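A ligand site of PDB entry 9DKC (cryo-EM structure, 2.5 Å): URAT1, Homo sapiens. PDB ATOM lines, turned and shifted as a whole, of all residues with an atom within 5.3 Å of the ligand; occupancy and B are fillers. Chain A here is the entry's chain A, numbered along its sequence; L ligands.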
ATOM      1  N   ILE A  28      32.281 -18.417   3.287  1.00  0.00           N
ATOM      2  CA  ILE A  28      31.449 -19.466   3.854  1.00  0.00           C
ATOM      3  C   ILE A  28      32.278 -20.632   4.380  1.00  0.00           C
ATOM      4  O   ILE A  28      31.873 -21.307   5.303  1.00  0.00           O
ATOM      5  CB  ILE A  28      30.369 -19.928   2.896  1.00  0.00           C
ATOM      6  CG1 ILE A  28      29.203 -18.959   2.957  1.00  0.00           C
ATOM      7  CG2 ILE A  28      29.841 -21.270   3.301  1.00  0.00           C
ATOM      8  CD1 ILE A  28      28.194 -19.194   1.872  1.00  0.00           C
ATOM      9  N   SER A  35      32.819 -22.215  13.088  1.00  0.00           N
ATOM     10  CA  SER A  35      31.871 -23.031  13.861  1.00  0.00           C
ATOM     11  C   SER A  35      32.464 -24.332  14.353  1.00  0.00           C
ATOM     12  O   SER A  35      32.162 -24.748  15.445  1.00  0.00           O
ATOM     13  CB  SER A  35      30.640 -23.385  13.032  1.00  0.00           C
ATOM     14  OG  SER A  35      29.826 -22.254  12.782  1.00  0.00           O
ATOM     15  N   LEU A 153      26.162 -21.040  20.343  1.00  0.00           N
ATOM     16  CA  LEU A 153      24.939 -21.305  19.581  1.00  0.00           C
ATOM     17  C   LEU A 153      23.845 -20.334  19.948  1.00  0.00           C
ATOM     18  O   LEU A 153      23.066 -19.961  19.118  1.00  0.00           O
ATOM     19  CB  LEU A 153      24.445 -22.714  19.798  1.00  0.00           C
ATOM     20  CG  LEU A 153      25.359 -23.720  19.144  1.00  0.00           C
ATOM     21  CD1 LEU A 153      24.883 -25.118  19.421  1.00  0.00           C
ATOM     22  CD2 LEU A 153      25.354 -23.429  17.677  1.00  0.00           C
ATOM     23  N   ILE A 156      23.944 -17.183  17.841  1.00  0.00           N
ATOM     24  CA  ILE A 156      23.362 -17.347  16.538  1.00  0.00           C
ATOM     25  C   ILE A 156      21.867 -17.124  16.558  1.00  0.00           C
ATOM     26  O   ILE A 156      21.345 -16.447  15.704  1.00  0.00           O
ATOM     27  CB  ILE A 156      23.683 -18.714  15.953  1.00  0.00           C
ATOM     28  CG1 ILE A 156      25.167 -18.801  15.720  1.00  0.00           C
ATOM     29  CG2 ILE A 156      22.995 -18.923  14.632  1.00  0.00           C
ATOM     30  CD1 ILE A 156      25.537 -19.656  14.544  1.00  0.00           C
ATOM     31  N   MET A 214      25.465 -15.139   7.535  1.00  0.00           N
ATOM     32  CA  MET A 214      24.747 -16.234   6.908  1.00  0.00           C
ATOM     33  C   MET A 214      23.441 -15.807   6.304  1.00  0.00           C
ATOM     34  O   MET A 214      23.095 -16.225   5.216  1.00  0.00           O
ATOM     35  CB  MET A 214      24.473 -17.345   7.894  1.00  0.00           C
ATOM     36  CG  MET A 214      25.484 -18.455   7.834  1.00  0.00           C
ATOM     37  SD  MET A 214      24.785 -19.862   8.669  1.00  0.00           S
ATOM     38  CE  MET A 214      25.015 -19.417  10.380  1.00  0.00           C
ATOM     39  N   THR A 217      24.252 -12.990   3.223  1.00  0.00           N
ATOM     40  CA  THR A 217      24.914 -13.549   2.059  1.00  0.00           C
ATOM     41  C   THR A 217      23.901 -14.274   1.231  1.00  0.00           C
ATOM     42  O   THR A 217      23.960 -14.177   0.030  1.00  0.00           O
ATOM     43  CB  THR A 217      26.199 -14.377   2.406  1.00  0.00           C
ATOM     44  OG1 THR A 217      27.198 -14.096   1.442  1.00  0.00           O
ATOM     45  CG2 THR A 217      26.004 -15.851   2.396  1.00  0.00           C
ATOM     46  N   MET A 234      22.058 -21.717  -4.906  1.00  0.00           N
ATOM     47  CA  MET A 234      21.903 -22.009  -3.484  1.00  0.00           C
ATOM     48  C   MET A 234      22.636 -23.289  -3.102  1.00  0.00           C
ATOM     49  O   MET A 234      23.268 -23.367  -2.034  1.00  0.00           O
ATOM     50  CB  MET A 234      20.410 -22.114  -3.135  1.00  0.00           C
ATOM     51  CG  MET A 234      19.947 -21.190  -2.005  1.00  0.00           C
ATOM     52  SD  MET A 234      20.532 -19.488  -2.149  1.00  0.00           S
ATOM     53  CE  MET A 234      19.941 -19.050  -3.778  1.00  0.00           C
ATOM     54  N   ASN A 237      26.182 -22.540  -2.718  1.00  0.00           N
ATOM     55  CA  ASN A 237      26.354 -21.860  -1.465  1.00  0.00           C
ATOM     56  C   ASN A 237      26.401 -22.887  -0.355  1.00  0.00           C
ATOM     57  O   ASN A 237      27.058 -22.698   0.635  1.00  0.00           O
ATOM     58  CB  ASN A 237      25.200 -20.928  -1.244  1.00  0.00           C
ATOM     59  CG  ASN A 237      25.571 -19.719  -0.501  1.00  0.00           C
ATOM     60  OD1 ASN A 237      26.514 -19.027  -0.864  1.00  0.00           O
ATOM     61  ND2 ASN A 237      24.836 -19.429   0.551  1.00  0.00           N
ATOM     62  N   SER A 238      25.681 -23.984  -0.519  1.00  0.00           N
ATOM     63  CA  SER A 238      25.675 -25.011   0.506  1.00  0.00           C
ATOM     64  C   SER A 238      26.926 -25.875   0.432  1.00  0.00           C
ATOM     65  O   SER A 238      27.408 -26.345   1.427  1.00  0.00           O
ATOM     66  CB  SER A 238      24.448 -25.884   0.398  1.00  0.00           C
ATOM     67  OG  SER A 238      24.232 -26.550   1.617  1.00  0.00           O
ATOM     68  N   PHE A 241      29.983 -24.417   2.291  1.00  0.00           N
ATOM     69  CA  PHE A 241      29.994 -24.715   3.707  1.00  0.00           C
ATOM     70  C   PHE A 241      30.425 -26.137   3.964  1.00  0.00           C
ATOM     71  O   PHE A 241      30.937 -26.424   5.025  1.00  0.00           O
ATOM     72  CB  PHE A 241      28.634 -24.488   4.318  1.00  0.00           C
ATOM     73  CG  PHE A 241      28.616 -24.585   5.803  1.00  0.00           C
ATOM     74  CD1 PHE A 241      28.518 -25.813   6.420  1.00  0.00           C
ATOM     75  CD2 PHE A 241      28.665 -23.456   6.579  1.00  0.00           C
ATOM     76  CE1 PHE A 241      28.497 -25.907   7.799  1.00  0.00           C
ATOM     77  CE2 PHE A 241      28.635 -23.546   7.956  1.00  0.00           C
ATOM     78  CZ  PHE A 241      28.551 -24.773   8.562  1.00  0.00           C
ATOM     79  N   PHE A 360      16.842 -32.238  13.316  1.00  0.00           N
ATOM     80  CA  PHE A 360      18.142 -32.083  12.663  1.00  0.00           C
ATOM     81  C   PHE A 360      18.990 -30.977  13.278  1.00  0.00           C
ATOM     82  O   PHE A 360      20.207 -31.023  13.216  1.00  0.00           O
ATOM     83  CB  PHE A 360      18.069 -31.778  11.169  1.00  0.00           C
ATOM     84  CG  PHE A 360      19.282 -31.030  10.687  1.00  0.00           C
ATOM     85  CD1 PHE A 360      20.444 -31.699  10.420  1.00  0.00           C
ATOM     86  CD2 PHE A 360      19.304 -29.667  10.689  1.00  0.00           C
ATOM     87  CE1 PHE A 360      21.576 -31.016  10.042  1.00  0.00           C
ATOM     88  CE2 PHE A 360      20.444 -28.979  10.340  1.00  0.00           C
ATOM     89  CZ  PHE A 360      21.580 -29.654  10.012  1.00  0.00           C
ATOM     90  N   GLY A 361      18.390 -29.925  13.784  1.00  0.00           N
ATOM     91  CA  GLY A 361      19.194 -28.881  14.356  1.00  0.00           C
ATOM     92  C   GLY A 361      19.830 -29.349  15.638  1.00  0.00           C
ATOM     93  O   GLY A 361      20.919 -28.983  15.954  1.00  0.00           O
ATOM     94  N   PHE A 364      22.487 -32.812  14.992  1.00  0.00           N
ATOM     95  CA  PHE A 364      23.681 -32.666  14.213  1.00  0.00           C
ATOM     96  C   PHE A 364      24.647 -31.797  14.867  1.00  0.00           C
ATOM     97  O   PHE A 364      25.823 -31.872  14.572  1.00  0.00           O
ATOM     98  CB  PHE A 364      23.377 -32.092  12.849  1.00  0.00           C
ATOM     99  CG  PHE A 364      24.576 -31.542  12.168  1.00  0.00           C
ATOM    100  CD1 PHE A 364      25.250 -32.276  11.242  1.00  0.00           C
ATOM    101  CD2 PHE A 364      25.024 -30.280  12.473  1.00  0.00           C
ATOM    102  CE1 PHE A 364      26.364 -31.769  10.616  1.00  0.00           C
ATOM    103  CE2 PHE A 364      26.129 -29.766  11.856  1.00  0.00           C
ATOM    104  CZ  PHE A 364      26.799 -30.512  10.922  1.00  0.00           C
ATOM    105  N   PHE A 365      24.174 -30.922  15.718  1.00  0.00           N
ATOM    106  CA  PHE A 365      25.116 -30.095  16.385  1.00  0.00           C
ATOM    107  C   PHE A 365      25.603 -30.825  17.562  1.00  0.00           C
ATOM    108  O   PHE A 365      26.738 -30.677  17.930  1.00  0.00           O
ATOM    109  CB  PHE A 365      24.580 -28.722  16.681  1.00  0.00           C
ATOM    110  CG  PHE A 365      24.812 -27.823  15.554  1.00  0.00           C
ATOM    111  CD1 PHE A 365      26.090 -27.603  15.142  1.00  0.00           C
ATOM    112  CD2 PHE A 365      23.762 -27.323  14.825  1.00  0.00           C
ATOM    113  CE1 PHE A 365      26.349 -26.822  14.055  1.00  0.00           C
ATOM    114  CE2 PHE A 365      24.012 -26.538  13.736  1.00  0.00           C
ATOM    115  CZ  PHE A 365      25.312 -26.287  13.346  1.00  0.00           C
ATOM    116  N   ASP A 389      30.123 -35.378   2.481  1.00  0.00           N
ATOM    117  CA  ASP A 389      28.946 -34.572   2.491  1.00  0.00           C
ATOM    118  C   ASP A 389      28.531 -34.191   1.115  1.00  0.00           C
ATOM    119  O   ASP A 389      27.354 -34.121   0.811  1.00  0.00           O
ATOM    120  CB  ASP A 389      29.200 -33.327   3.304  1.00  0.00           C
ATOM    121  CG  ASP A 389      28.121 -33.048   4.313  1.00  0.00           C
ATOM    122  OD1 ASP A 389      26.960 -33.417   4.017  1.00  0.00           O
ATOM    123  OD2 ASP A 389      28.412 -32.467   5.378  1.00  0.00           O
ATOM    124  N   LYS A 393      24.812 -34.726  -0.881  1.00  0.00           N
ATOM    125  CA  LYS A 393      24.089 -33.502  -1.276  1.00  0.00           C
ATOM    126  C   LYS A 393      23.834 -33.419  -2.772  1.00  0.00           C
ATOM    127  O   LYS A 393      22.927 -32.747  -3.208  1.00  0.00           O
ATOM    128  CB  LYS A 393      24.849 -32.259  -0.886  1.00  0.00           C
ATOM    129  CG  LYS A 393      24.734 -31.860   0.560  1.00  0.00           C
ATOM    130  CD  LYS A 393      25.496 -30.576   0.789  1.00  0.00           C
ATOM    131  CE  LYS A 393      25.636 -30.264   2.268  1.00  0.00           C
ATOM    132  NZ  LYS A 393      25.600 -28.804   2.552  1.00  0.00           N
ATOM    133  N   GLY A 446      23.142 -34.533   6.922  1.00  0.00           N
ATOM    134  CA  GLY A 446      23.348 -33.459   5.968  1.00  0.00           C
ATOM    135  C   GLY A 446      22.370 -33.550   4.836  1.00  0.00           C
ATOM    136  O   GLY A 446      21.800 -32.571   4.439  1.00  0.00           O
ATOM    137  N   PHE A 449      18.866 -32.604   5.913  1.00  0.00           N
ATOM    138  CA  PHE A 449      18.769 -31.158   6.054  1.00  0.00           C
ATOM    139  C   PHE A 449      18.580 -30.464   4.736  1.00  0.00           C
ATOM    140  O   PHE A 449      17.885 -29.487   4.676  1.00  0.00           O
ATOM    141  CB  PHE A 449      19.982 -30.530   6.686  1.00  0.00           C
ATOM    142  CG  PHE A 449      20.088 -29.069   6.404  1.00  0.00           C
ATOM    143  CD1 PHE A 449      19.339 -28.166   7.115  1.00  0.00           C
ATOM    144  CD2 PHE A 449      20.898 -28.608   5.399  1.00  0.00           C
ATOM    145  CE1 PHE A 449      19.418 -26.826   6.851  1.00  0.00           C
ATOM    146  CE2 PHE A 449      20.981 -27.263   5.123  1.00  0.00           C
ATOM    147  CZ  PHE A 449      20.237 -26.366   5.858  1.00  0.00           C
ATOM    148  N   ALA A 476      14.909 -25.085  14.457  1.00  0.00           N
ATOM    149  CA  ALA A 476      16.165 -25.734  14.153  1.00  0.00           C
ATOM    150  C   ALA A 476      17.287 -25.061  14.853  1.00  0.00           C
ATOM    151  O   ALA A 476      18.300 -25.685  15.064  1.00  0.00           O
ATOM    152  CB  ALA A 476      16.443 -25.744  12.685  1.00  0.00           C
ATOM    153  N   ARG A 477      17.167 -23.790  15.178  1.00  0.00           N
ATOM    154  CA  ARG A 477      18.245 -23.153  15.910  1.00  0.00           C
ATOM    155  C   ARG A 477      18.104 -23.501  17.362  1.00  0.00           C
ATOM    156  O   ARG A 477      19.077 -23.822  17.978  1.00  0.00           O
ATOM    157  CB  ARG A 477      18.313 -21.668  15.714  1.00  0.00           C
ATOM    158  CG  ARG A 477      19.211 -21.332  14.573  1.00  0.00           C
ATOM    159  CD  ARG A 477      19.080 -19.877  14.215  1.00  0.00           C
ATOM    160  NE  ARG A 477      19.101 -19.708  12.779  1.00  0.00           N
ATOM    161  CZ  ARG A 477      18.184 -19.045  12.114  1.00  0.00           C
ATOM    162  NH1 ARG A 477      17.188 -18.479  12.765  1.00  0.00           N
ATOM    163  NH2 ARG A 477      18.275 -18.941  10.806  1.00  0.00           N
ATOM    164  N   ALA A 480      19.529 -26.709  18.162  1.00  0.00           N
ATOM    165  CA  ALA A 480      20.960 -26.678  18.173  1.00  0.00           C
ATOM    166  C   ALA A 480      21.409 -26.231  19.517  1.00  0.00           C
ATOM    167  O   ALA A 480      22.261 -26.853  20.094  1.00  0.00           O
ATOM    168  CB  ALA A 480      21.490 -25.765  17.098  1.00  0.00           C
HETATM  169  C1  LIG L   1      23.591 -20.437   5.439  1.00  0.00           C
HETATM  170  C2  LIG L   1      24.872 -20.934   3.431  1.00  0.00           C
HETATM  171  C3  LIG L   1      23.823 -23.866   8.781  1.00  0.00           C
HETATM  172  C4  LIG L   1      25.870 -21.600   5.521  1.00  0.00           C
HETATM  173  C5  LIG L   1      24.545 -21.445   4.807  1.00  0.00           C
HETATM  174  C6  LIG L   1      24.166 -24.528   5.402  1.00  0.00           C
HETATM  175  C7  LIG L   1      24.520 -26.638   5.727  1.00  0.00           C
HETATM  176  C8  LIG L   1      24.779 -25.977   6.882  1.00  0.00           C
HETATM  177  C9  LIG L   1      24.722 -23.634   7.611  1.00  0.00           C
HETATM  178  C10 LIG L   1      22.587 -24.383   8.523  1.00  0.00           C
HETATM  179  C11 LIG L   1      21.734 -24.586   9.568  1.00  0.00           C
HETATM  180  C12 LIG L   1      22.136 -24.267  10.838  1.00  0.00           C
HETATM  181  C13 LIG L   1      23.395 -23.753  11.086  1.00  0.00           C
HETATM  182  C14 LIG L   1      23.770 -23.437  12.378  1.00  0.00           C
HETATM  183  C15 LIG L   1      25.016 -22.905  12.621  1.00  0.00           C
HETATM  184  C16 LIG L   1      25.891 -22.703  11.576  1.00  0.00           C
HETATM  185  C17 LIG L   1      25.498 -23.007  10.291  1.00  0.00           C
HETATM  186  C18 LIG L   1      24.230 -23.536  10.058  1.00  0.00           C
HETATM  187  C19 LIG L   1      25.204 -26.724   7.979  1.00  0.00           C
HETATM  188  C20 LIG L   1      25.340 -28.090   7.822  1.00  0.00           C
HETATM  189  C21 LIG L   1      25.056 -28.684   6.614  1.00  0.00           C
HETATM  190  N1  LIG L   1      24.141 -25.715   4.847  1.00  0.00           N
HETATM  191  N2  LIG L   1      24.549 -24.687   6.651  1.00  0.00           N
HETATM  192  N3  LIG L   1      24.661 -27.958   5.609  1.00  0.00           N
HETATM  193  O1  LIG L   1      24.841 -21.750   2.490  1.00  0.00           O
HETATM  194  O2  LIG L   1      25.148 -19.712   3.262  1.00  0.00           O
HETATM  195  S1  LIG L   1      23.683 -23.011   4.523  1.00  0.00           S
HETATM  196 BR1  LIG L   1      20.917 -24.568  12.257  1.00  0.00          BR
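OG of Ser 238 lies within hydrogen-bond range of N1 of the ligand (3.3 Å).
An oxygen (O2) of the ligand is in hydrogen-bond range of the side-chain amide nitrogen of Asn 237, at 2.7 Å.
An oxygen (O1) of the ligand lies close to the backbone carbonyl oxygen of Asn 237 (3.0 Å).
The side-chain amino group (NZ) of Lys 393 is in hydrogen-bond range of a nitrogen (N3) of the ligand, 3.3 Å away.
NZ of Lys 393 lies within hydrogen-bond range of OG of Ser 238, 2.8 Å away.
Merely in contact with the ligand: Ile 28, Ile 156, Met 214, Phe 241, Phe 365, Phe 449 and Ala 476.
Hydrophobic or aromatic side chains within 4 Å of the ligand: Ile 28, Ile 156, Met 214, Phe 241, Phe 365 and Phe 449.
Within 4 Å of the ligand: Ile 28, Ile 156, Met 214, Asn 237, Ser 238, Phe 241, Phe 365, Lys 393, Phe 449 and Ala 476.
The nearest printed residue that does not touch the ligand is Thr 217 (4.05 Å).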
